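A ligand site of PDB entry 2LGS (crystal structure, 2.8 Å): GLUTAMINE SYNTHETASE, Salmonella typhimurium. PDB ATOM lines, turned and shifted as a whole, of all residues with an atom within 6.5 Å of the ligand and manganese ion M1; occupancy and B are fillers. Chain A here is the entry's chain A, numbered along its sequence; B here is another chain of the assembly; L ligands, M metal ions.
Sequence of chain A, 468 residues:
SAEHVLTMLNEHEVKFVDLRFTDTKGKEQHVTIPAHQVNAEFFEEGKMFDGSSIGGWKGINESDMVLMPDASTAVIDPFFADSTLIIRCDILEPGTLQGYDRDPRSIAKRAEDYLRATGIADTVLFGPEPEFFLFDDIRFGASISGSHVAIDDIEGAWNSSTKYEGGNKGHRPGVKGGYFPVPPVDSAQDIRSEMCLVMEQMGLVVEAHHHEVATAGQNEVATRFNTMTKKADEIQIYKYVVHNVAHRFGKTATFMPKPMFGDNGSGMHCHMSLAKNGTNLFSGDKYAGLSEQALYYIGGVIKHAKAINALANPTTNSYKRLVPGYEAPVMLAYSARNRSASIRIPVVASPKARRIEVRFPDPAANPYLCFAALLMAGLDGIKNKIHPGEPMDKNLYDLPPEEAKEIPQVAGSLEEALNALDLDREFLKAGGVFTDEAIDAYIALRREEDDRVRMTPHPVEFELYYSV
Gly 267 touches the ligand. Of the 24 residues printed, 9 come within 4 Å of the ligand. Along chain A the residues within 4 Å of the ligand span positions 131 to 359. The nearest printed residue that does not touch the ligand is Ser 266 (4.3 Å).
OE1 of Glu 131 lies within hydrogen-bond range of N of Gly 267. The backbone carbonyl oxygen of Glu 212 lies within hydrogen-bond range of the backbone NH of Tyr 179. O of Gly 265 lies within hydrogen-bond range of NE2 of Gln 218 (2.8 Å). The backbone carbonyl oxygen of His 269 is in hydrogen-bond range of the backbone NH of Glu 129 (2.8 Å). O of Arg 359 is in hydrogen-bond range of NH2 of Arg 321 (3.1 Å). O of Gln 218 sits at hydrogen-bond distance from N of Glu 212 (2.8 Å). A ring nitrogen (ND1) of His 269 lies within hydrogen-bond range of the side-chain carboxylate (OE1) of Glu 357 (3.1 Å). The backbone NH (N) of His 210 is in hydrogen-bond range of the backbone carbonyl oxygen (O) of Glu 220.
A nitrogen (N1) of the ligand is in hydrogen-bond range of the backbone carbonyl oxygen (O) of Gly 265, at 2.9 Å. An oxygen (O2) of the ligand lies within salt-bridge range of the guanidinium group of Arg 359 (2.4 Å). A nitrogen (N1) of the ligand sits at hydrogen-bond distance from the side-chain amide oxygen (OD1) of Asn 264 (2.7 Å). A nitrogen (N1) of the ligand lies within salt-bridge range of the side-chain carboxylate of Glu 131 (2.7 Å). O2 of the ligand is in salt-bridge range of NH2 of Arg 339 (3.6 Å). NE of Arg 321 lies within salt-bridge range of O1 of the ligand, 2.8 Å away. O4 of the ligand sits at hydrogen-bond distance from NE2 of His 269 (3.4 Å).
Manganese ion M1 is bound by OE1 of Glu 220. Manganese ion M1 is bound by the side-chain carboxylate (OE2) of Glu 131, at 2.2 Å. Manganese ion M1 is bound by the side-chain carboxylate (OE2) of Glu 212, at 2.3 Å. Manganese ion M1 has three donor atoms within binding distance.
Of the 24 residues printed, 3 come within 4 Å of manganese ion M1. The nearest printed residue that does not touch manganese ion M1 is His 210 (4.7 Å).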
ATOM      1  N   GLU A 129      20.406  -9.936 -18.700  1.00  0.00           N
ATOM      2  CA  GLU A 129      20.523 -10.068 -20.161  1.00  0.00           C
ATOM      3  C   GLU A 129      19.108 -10.226 -20.762  1.00  0.00           C
ATOM      4  O   GLU A 129      18.744 -11.361 -21.140  1.00  0.00           O
ATOM      5  CB  GLU A 129      21.396 -11.310 -20.509  1.00  0.00           C
ATOM      6  CG  GLU A 129      22.778 -11.553 -19.869  1.00  0.00           C
ATOM      7  CD  GLU A 129      23.449 -12.922 -20.203  1.00  0.00           C
ATOM      8  OE1 GLU A 129      22.900 -13.981 -19.849  1.00  0.00           O
ATOM      9  OE2 GLU A 129      24.561 -12.942 -20.777  1.00  0.00           O
ATOM     10  N   PRO A 130      18.240  -9.208 -20.819  1.00  0.00           N
ATOM     11  CA  PRO A 130      16.853  -9.322 -21.260  1.00  0.00           C
ATOM     12  C   PRO A 130      16.710  -9.586 -22.739  1.00  0.00           C
ATOM     13  O   PRO A 130      17.369  -8.972 -23.557  1.00  0.00           O
ATOM     14  CB  PRO A 130      16.189  -8.026 -20.905  1.00  0.00           C
ATOM     15  CG  PRO A 130      17.184  -7.334 -20.038  1.00  0.00           C
ATOM     16  CD  PRO A 130      18.510  -7.807 -20.612  1.00  0.00           C
ATOM     17  N   GLU A 131      15.890 -10.559 -23.112  1.00  0.00           N
ATOM     18  CA  GLU A 131      15.606 -10.758 -24.527  1.00  0.00           C
ATOM     19  C   GLU A 131      14.183 -10.349 -24.869  1.00  0.00           C
ATOM     20  O   GLU A 131      13.277 -10.332 -24.031  1.00  0.00           O
ATOM     21  CB  GLU A 131      15.787 -12.186 -24.891  1.00  0.00           C
ATOM     22  CG  GLU A 131      17.207 -12.599 -24.662  1.00  0.00           C
ATOM     23  CD  GLU A 131      17.371 -14.101 -24.537  1.00  0.00           C
ATOM     24  OE1 GLU A 131      16.593 -14.796 -23.873  1.00  0.00           O
ATOM     25  OE2 GLU A 131      18.322 -14.594 -25.141  1.00  0.00           O
ATOM     26  N   TYR A 179      19.844 -17.256 -34.793  1.00  0.00           N
ATOM     27  CA  TYR A 179      21.176 -17.022 -34.284  1.00  0.00           C
ATOM     28  C   TYR A 179      22.332 -16.966 -35.285  1.00  0.00           C
ATOM     29  O   TYR A 179      22.947 -17.900 -35.791  1.00  0.00           O
ATOM     30  CB  TYR A 179      21.508 -18.050 -33.233  1.00  0.00           C
ATOM     31  CG  TYR A 179      22.447 -17.445 -32.212  1.00  0.00           C
ATOM     32  CD1 TYR A 179      21.946 -16.659 -31.171  1.00  0.00           C
ATOM     33  CD2 TYR A 179      23.821 -17.689 -32.312  1.00  0.00           C
ATOM     34  CE1 TYR A 179      22.828 -16.126 -30.225  1.00  0.00           C
ATOM     35  CE2 TYR A 179      24.709 -17.175 -31.376  1.00  0.00           C
ATOM     36  CZ  TYR A 179      24.205 -16.385 -30.344  1.00  0.00           C
ATOM     37  OH  TYR A 179      25.096 -15.844 -29.418  1.00  0.00           O
ATOM     38  N   HIS A 210      22.492  -8.173 -30.866  1.00  0.00           N
ATOM     39  CA  HIS A 210      22.399  -9.200 -31.881  1.00  0.00           C
ATOM     40  C   HIS A 210      21.043  -9.863 -31.937  1.00  0.00           C
ATOM     41  O   HIS A 210      20.285  -9.841 -30.954  1.00  0.00           O
ATOM     42  CB  HIS A 210      23.420 -10.283 -31.643  1.00  0.00           C
ATOM     43  CG  HIS A 210      23.230 -10.965 -30.308  1.00  0.00           C
ATOM     44  ND1 HIS A 210      22.535 -12.056 -30.056  1.00  0.00           N
ATOM     45  CD2 HIS A 210      23.755 -10.524 -29.124  1.00  0.00           C
ATOM     46  CE1 HIS A 210      22.615 -12.278 -28.782  1.00  0.00           C
ATOM     47  NE2 HIS A 210      23.347 -11.362 -28.233  1.00  0.00           N
ATOM     48  N   GLU A 212      18.571 -13.035 -31.717  1.00  0.00           N
ATOM     49  CA  GLU A 212      18.608 -14.247 -30.913  1.00  0.00           C
ATOM     50  C   GLU A 212      18.174 -15.504 -31.656  1.00  0.00           C
ATOM     51  O   GLU A 212      17.912 -15.413 -32.855  1.00  0.00           O
ATOM     52  CB  GLU A 212      17.756 -14.037 -29.675  1.00  0.00           C
ATOM     53  CG  GLU A 212      18.651 -13.868 -28.447  1.00  0.00           C
ATOM     54  CD  GLU A 212      19.537 -15.070 -28.061  1.00  0.00           C
ATOM     55  OE1 GLU A 212      19.232 -16.217 -28.403  1.00  0.00           O
ATOM     56  OE2 GLU A 212      20.550 -14.868 -27.365  1.00  0.00           O
ATOM     57  N   VAL A 213      18.041 -16.650 -31.017  1.00  0.00           N
ATOM     58  CA  VAL A 213      17.811 -17.925 -31.660  1.00  0.00           C
ATOM     59  C   VAL A 213      16.518 -18.093 -32.430  1.00  0.00           C
ATOM     60  O   VAL A 213      16.474 -18.721 -33.479  1.00  0.00           O
ATOM     61  CB  VAL A 213      17.960 -18.988 -30.558  1.00  0.00           C
ATOM     62  CG1 VAL A 213      17.268 -20.305 -30.848  1.00  0.00           C
ATOM     63  CG2 VAL A 213      19.437 -19.325 -30.511  1.00  0.00           C
ATOM     64  N   GLN A 218      13.348 -12.645 -32.596  1.00  0.00           N
ATOM     65  CA  GLN A 218      13.918 -12.577 -31.254  1.00  0.00           C
ATOM     66  C   GLN A 218      15.190 -11.749 -31.283  1.00  0.00           C
ATOM     67  O   GLN A 218      16.042 -11.920 -32.166  1.00  0.00           O
ATOM     68  CB  GLN A 218      14.248 -13.934 -30.723  1.00  0.00           C
ATOM     69  CG  GLN A 218      14.050 -13.828 -29.209  1.00  0.00           C
ATOM     70  CD  GLN A 218      14.438 -15.081 -28.465  1.00  0.00           C
ATOM     71  OE1 GLN A 218      15.196 -15.919 -28.963  1.00  0.00           O
ATOM     72  NE2 GLN A 218      13.916 -15.223 -27.243  1.00  0.00           N
ATOM     73  N   GLU A 220      18.318  -9.148 -28.908  1.00  0.00           N
ATOM     74  CA  GLU A 220      18.991  -8.851 -27.646  1.00  0.00           C
ATOM     75  C   GLU A 220      19.934  -7.669 -27.749  1.00  0.00           C
ATOM     76  O   GLU A 220      20.791  -7.610 -28.630  1.00  0.00           O
ATOM     77  CB  GLU A 220      19.758 -10.052 -27.208  1.00  0.00           C
ATOM     78  CG  GLU A 220      20.182 -10.028 -25.749  1.00  0.00           C
ATOM     79  CD  GLU A 220      20.908 -11.311 -25.350  1.00  0.00           C
ATOM     80  OE1 GLU A 220      20.620 -12.340 -25.946  1.00  0.00           O
ATOM     81  OE2 GLU A 220      21.761 -11.300 -24.463  1.00  0.00           O
ATOM     82  N   PRO A 257       7.701 -14.166 -21.750  1.00  0.00           N
ATOM     83  CA  PRO A 257       8.722 -15.214 -21.699  1.00  0.00           C
ATOM     84  C   PRO A 257       8.666 -16.226 -22.840  1.00  0.00           C
ATOM     85  O   PRO A 257       9.653 -16.643 -23.428  1.00  0.00           O
ATOM     86  CB  PRO A 257       8.513 -15.859 -20.376  1.00  0.00           C
ATOM     87  CG  PRO A 257       7.734 -14.831 -19.585  1.00  0.00           C
ATOM     88  CD  PRO A 257       6.812 -14.241 -20.598  1.00  0.00           C
ATOM     89  N   ASN A 264      12.511 -20.842 -29.302  1.00  0.00           N
ATOM     90  CA  ASN A 264      13.015 -20.153 -28.136  1.00  0.00           C
ATOM     91  C   ASN A 264      12.103 -19.164 -27.398  1.00  0.00           C
ATOM     92  O   ASN A 264      11.243 -18.477 -27.955  1.00  0.00           O
ATOM     93  CB  ASN A 264      14.289 -19.459 -28.563  1.00  0.00           C
ATOM     94  CG  ASN A 264      15.379 -19.495 -27.510  1.00  0.00           C
ATOM     95  OD1 ASN A 264      15.996 -18.498 -27.132  1.00  0.00           O
ATOM     96  ND2 ASN A 264      15.695 -20.670 -27.005  1.00  0.00           N
ATOM     97  N   GLY A 265      12.359 -19.120 -26.102  1.00  0.00           N
ATOM     98  CA  GLY A 265      11.696 -18.173 -25.230  1.00  0.00           C
ATOM     99  C   GLY A 265      12.664 -17.045 -24.879  1.00  0.00           C
ATOM    100  O   GLY A 265      13.883 -17.073 -25.079  1.00  0.00           O
ATOM    101  N   SER A 266      12.103 -15.970 -24.402  1.00  0.00           N
ATOM    102  CA  SER A 266      12.893 -14.842 -23.974  1.00  0.00           C
ATOM    103  C   SER A 266      13.171 -14.947 -22.481  1.00  0.00           C
ATOM    104  O   SER A 266      12.282 -14.895 -21.620  1.00  0.00           O
ATOM    105  CB  SER A 266      12.143 -13.563 -24.290  1.00  0.00           C
ATOM    106  OG  SER A 266      12.077 -13.376 -25.697  1.00  0.00           O
ATOM    107  N   GLY A 267      14.426 -15.176 -22.140  1.00  0.00           N
ATOM    108  CA  GLY A 267      14.848 -15.135 -20.752  1.00  0.00           C
ATOM    109  C   GLY A 267      15.654 -13.895 -20.390  1.00  0.00           C
ATOM    110  O   GLY A 267      16.227 -13.208 -21.255  1.00  0.00           O
ATOM    111  N   MET A 268      15.740 -13.545 -19.117  1.00  0.00           N
ATOM    112  CA  MET A 268      16.545 -12.426 -18.652  1.00  0.00           C
ATOM    113  C   MET A 268      17.528 -12.966 -17.619  1.00  0.00           C
ATOM    114  O   MET A 268      17.271 -13.002 -16.425  1.00  0.00           O
ATOM    115  CB  MET A 268      15.673 -11.365 -17.980  1.00  0.00           C
ATOM    116  CG  MET A 268      16.396 -10.109 -17.534  1.00  0.00           C
ATOM    117  SD  MET A 268      15.446  -9.373 -16.180  1.00  0.00           S
ATOM    118  CE  MET A 268      14.682  -8.024 -17.024  1.00  0.00           C
ATOM    119  N   HIS A 269      18.702 -13.404 -18.060  1.00  0.00           N
ATOM    120  CA  HIS A 269      19.660 -13.960 -17.108  1.00  0.00           C
ATOM    121  C   HIS A 269      20.313 -12.896 -16.270  1.00  0.00           C
ATOM    122  O   HIS A 269      20.869 -11.942 -16.808  1.00  0.00           O
ATOM    123  CB  HIS A 269      20.830 -14.689 -17.714  1.00  0.00           C
ATOM    124  CG  HIS A 269      20.526 -15.767 -18.745  1.00  0.00           C
ATOM    125  ND1 HIS A 269      21.368 -16.708 -19.175  1.00  0.00           N
ATOM    126  CD2 HIS A 269      19.301 -15.951 -19.348  1.00  0.00           C
ATOM    127  CE1 HIS A 269      20.645 -17.434 -20.001  1.00  0.00           C
ATOM    128  NE2 HIS A 269      19.442 -16.996 -20.103  1.00  0.00           N
ATOM    129  N   ARG A 321       8.298 -21.581 -20.660  1.00  0.00           N
ATOM    130  CA  ARG A 321       9.724 -21.514 -20.981  1.00  0.00           C
ATOM    131  C   ARG A 321      10.510 -22.464 -20.096  1.00  0.00           C
ATOM    132  O   ARG A 321      11.384 -23.217 -20.539  1.00  0.00           O
ATOM    133  CB  ARG A 321      10.227 -20.081 -20.771  1.00  0.00           C
ATOM    134  CG  ARG A 321      11.744 -19.934 -20.775  1.00  0.00           C
ATOM    135  CD  ARG A 321      12.211 -18.492 -20.811  1.00  0.00           C
ATOM    136  NE  ARG A 321      13.629 -18.393 -20.463  1.00  0.00           N
ATOM    137  CZ  ARG A 321      14.002 -18.294 -19.183  1.00  0.00           C
ATOM    138  NH1 ARG A 321      13.097 -18.189 -18.193  1.00  0.00           N
ATOM    139  NH2 ARG A 321      15.287 -18.264 -18.889  1.00  0.00           N
ATOM    140  N   PRO A 329      16.579 -24.109 -18.633  1.00  0.00           N
ATOM    141  CA  PRO A 329      17.447 -24.107 -17.462  1.00  0.00           C
ATOM    142  C   PRO A 329      16.701 -24.451 -16.174  1.00  0.00           C
ATOM    143  O   PRO A 329      16.601 -23.665 -15.221  1.00  0.00           O
ATOM    144  CB  PRO A 329      18.070 -22.721 -17.461  1.00  0.00           C
ATOM    145  CG  PRO A 329      16.922 -21.843 -17.850  1.00  0.00           C
ATOM    146  CD  PRO A 329      16.292 -22.704 -18.962  1.00  0.00           C
ATOM    147  N   ARG A 339      25.529 -26.191 -19.424  1.00  0.00           N
ATOM    148  CA  ARG A 339      24.435 -25.250 -19.753  1.00  0.00           C
ATOM    149  C   ARG A 339      23.179 -26.132 -19.922  1.00  0.00           C
ATOM    150  O   ARG A 339      22.833 -26.722 -20.947  1.00  0.00           O
ATOM    151  CB  ARG A 339      24.646 -24.444 -21.072  1.00  0.00           C
ATOM    152  CG  ARG A 339      25.896 -23.564 -21.251  1.00  0.00           C
ATOM    153  CD  ARG A 339      25.768 -22.028 -21.369  1.00  0.00           C
ATOM    154  NE  ARG A 339      25.134 -21.435 -22.553  1.00  0.00           N
ATOM    155  CZ  ARG A 339      25.536 -20.258 -23.087  1.00  0.00           C
ATOM    156  NH1 ARG A 339      26.633 -19.614 -22.706  1.00  0.00           N
ATOM    157  NH2 ARG A 339      24.808 -19.695 -24.048  1.00  0.00           N
ATOM    158  N   GLU A 357      26.179 -16.446 -12.795  1.00  0.00           N
ATOM    159  CA  GLU A 357      25.065 -16.106 -13.672  1.00  0.00           C
ATOM    160  C   GLU A 357      23.842 -16.974 -13.403  1.00  0.00           C
ATOM    161  O   GLU A 357      23.864 -18.183 -13.629  1.00  0.00           O
ATOM    162  CB  GLU A 357      25.476 -16.289 -15.127  1.00  0.00           C
ATOM    163  CG  GLU A 357      24.382 -15.718 -16.005  1.00  0.00           C
ATOM    164  CD  GLU A 357      24.489 -16.171 -17.439  1.00  0.00           C
ATOM    165  OE1 GLU A 357      24.090 -17.283 -17.743  1.00  0.00           O
ATOM    166  OE2 GLU A 357      24.968 -15.407 -18.258  1.00  0.00           O
ATOM    167  N   ARG A 359      20.640 -18.263 -14.773  1.00  0.00           N
ATOM    168  CA  ARG A 359      19.972 -18.324 -16.065  1.00  0.00           C
ATOM    169  C   ARG A 359      18.457 -18.377 -16.098  1.00  0.00           C
ATOM    170  O   ARG A 359      17.876 -18.062 -17.129  1.00  0.00           O
ATOM    171  CB  ARG A 359      20.440 -19.523 -16.846  1.00  0.00           C
ATOM    172  CG  ARG A 359      21.893 -19.475 -17.215  1.00  0.00           C
ATOM    173  CD  ARG A 359      22.030 -20.484 -18.301  1.00  0.00           C
ATOM    174  NE  ARG A 359      22.886 -19.976 -19.361  1.00  0.00           N
ATOM    175  CZ  ARG A 359      22.493 -19.891 -20.632  1.00  0.00           C
ATOM    176  NH1 ARG A 359      21.240 -20.076 -21.071  1.00  0.00           N
ATOM    177  NH2 ARG A 359      23.362 -19.503 -21.525  1.00  0.00           N
ATOM    178  N   PHE A 360      17.784 -18.703 -15.001  1.00  0.00           N
ATOM    179  CA  PHE A 360      16.344 -18.864 -15.045  1.00  0.00           C
ATOM    180  C   PHE A 360      15.371 -17.692 -15.019  1.00  0.00           C
ATOM    181  O   PHE A 360      14.215 -17.945 -15.332  1.00  0.00           O
ATOM    182  CB  PHE A 360      15.904 -19.859 -13.936  1.00  0.00           C
ATOM    183  CG  PHE A 360      16.046 -19.443 -12.467  1.00  0.00           C
ATOM    184  CD1 PHE A 360      15.208 -18.490 -11.887  1.00  0.00           C
ATOM    185  CD2 PHE A 360      17.015 -20.058 -11.668  1.00  0.00           C
ATOM    186  CE1 PHE A 360      15.352 -18.128 -10.544  1.00  0.00           C
ATOM    187  CE2 PHE A 360      17.153 -19.689 -10.320  1.00  0.00           C
ATOM    188  CZ  PHE A 360      16.320 -18.738  -9.753  1.00  0.00           C
ATOM    189  N   PRO A 361      15.611 -16.446 -14.593  1.00  0.00           N
ATOM    190  CA  PRO A 361      14.577 -15.393 -14.605  1.00  0.00           C
ATOM    191  C   PRO A 361      14.166 -14.953 -16.015  1.00  0.00           C
ATOM    192  O   PRO A 361      14.862 -15.234 -16.999  1.00  0.00           O
ATOM    193  CB  PRO A 361      15.197 -14.256 -13.805  1.00  0.00           C
ATOM    194  CG  PRO A 361      16.212 -14.968 -12.982  1.00  0.00           C
ATOM    195  CD  PRO A 361      16.814 -15.983 -13.937  1.00  0.00           C
ATOM    196  N   ASP B  50      28.708 -17.290 -27.170  1.00  0.00           N
ATOM    197  CA  ASP B  50      28.290 -18.661 -27.091  1.00  0.00           C
ATOM    198  C   ASP B  50      28.253 -19.339 -28.468  1.00  0.00           C
ATOM    199  O   ASP B  50      27.315 -19.276 -29.266  1.00  0.00           O
ATOM    200  CB  ASP B  50      26.932 -18.773 -26.448  1.00  0.00           C
ATOM    201  CG  ASP B  50      26.551 -20.243 -26.288  1.00  0.00           C
ATOM    202  OD1 ASP B  50      27.288 -20.971 -25.606  1.00  0.00           O
ATOM    203  OD2 ASP B  50      25.522 -20.648 -26.836  1.00  0.00           O
HETATM  204  N1  LIG L   1      16.747 -17.333 -24.788  1.00  0.00           N
HETATM  205  C1  LIG L   1      17.146 -18.306 -23.785  1.00  0.00           C
HETATM  206  C2  LIG L   1      16.187 -18.402 -22.592  1.00  0.00           C
HETATM  207  O1  LIG L   1      15.020 -18.787 -22.850  1.00  0.00           O
HETATM  208  C3  LIG L   1      18.524 -17.925 -23.299  1.00  0.00           C
HETATM  209  C4  LIG L   1      19.525 -18.045 -24.444  1.00  0.00           C
HETATM  210  C5  LIG L   1      21.004 -18.090 -24.074  1.00  0.00           C
HETATM  211  O2  LIG L   1      21.400 -18.847 -23.175  1.00  0.00           O
HETATM  212  O3  LIG L   1      21.742 -17.378 -24.755  1.00  0.00           O
HETATM  213  O4  LIG L   1      16.575 -18.163 -21.443  1.00  0.00           O
HETATM  214 MN    MN M   1      20.527 -14.290 -25.118  1.00  0.00          MN
HETATM  215 MN    MN M   2      24.046 -15.789 -20.476  1.00  0.00          MN
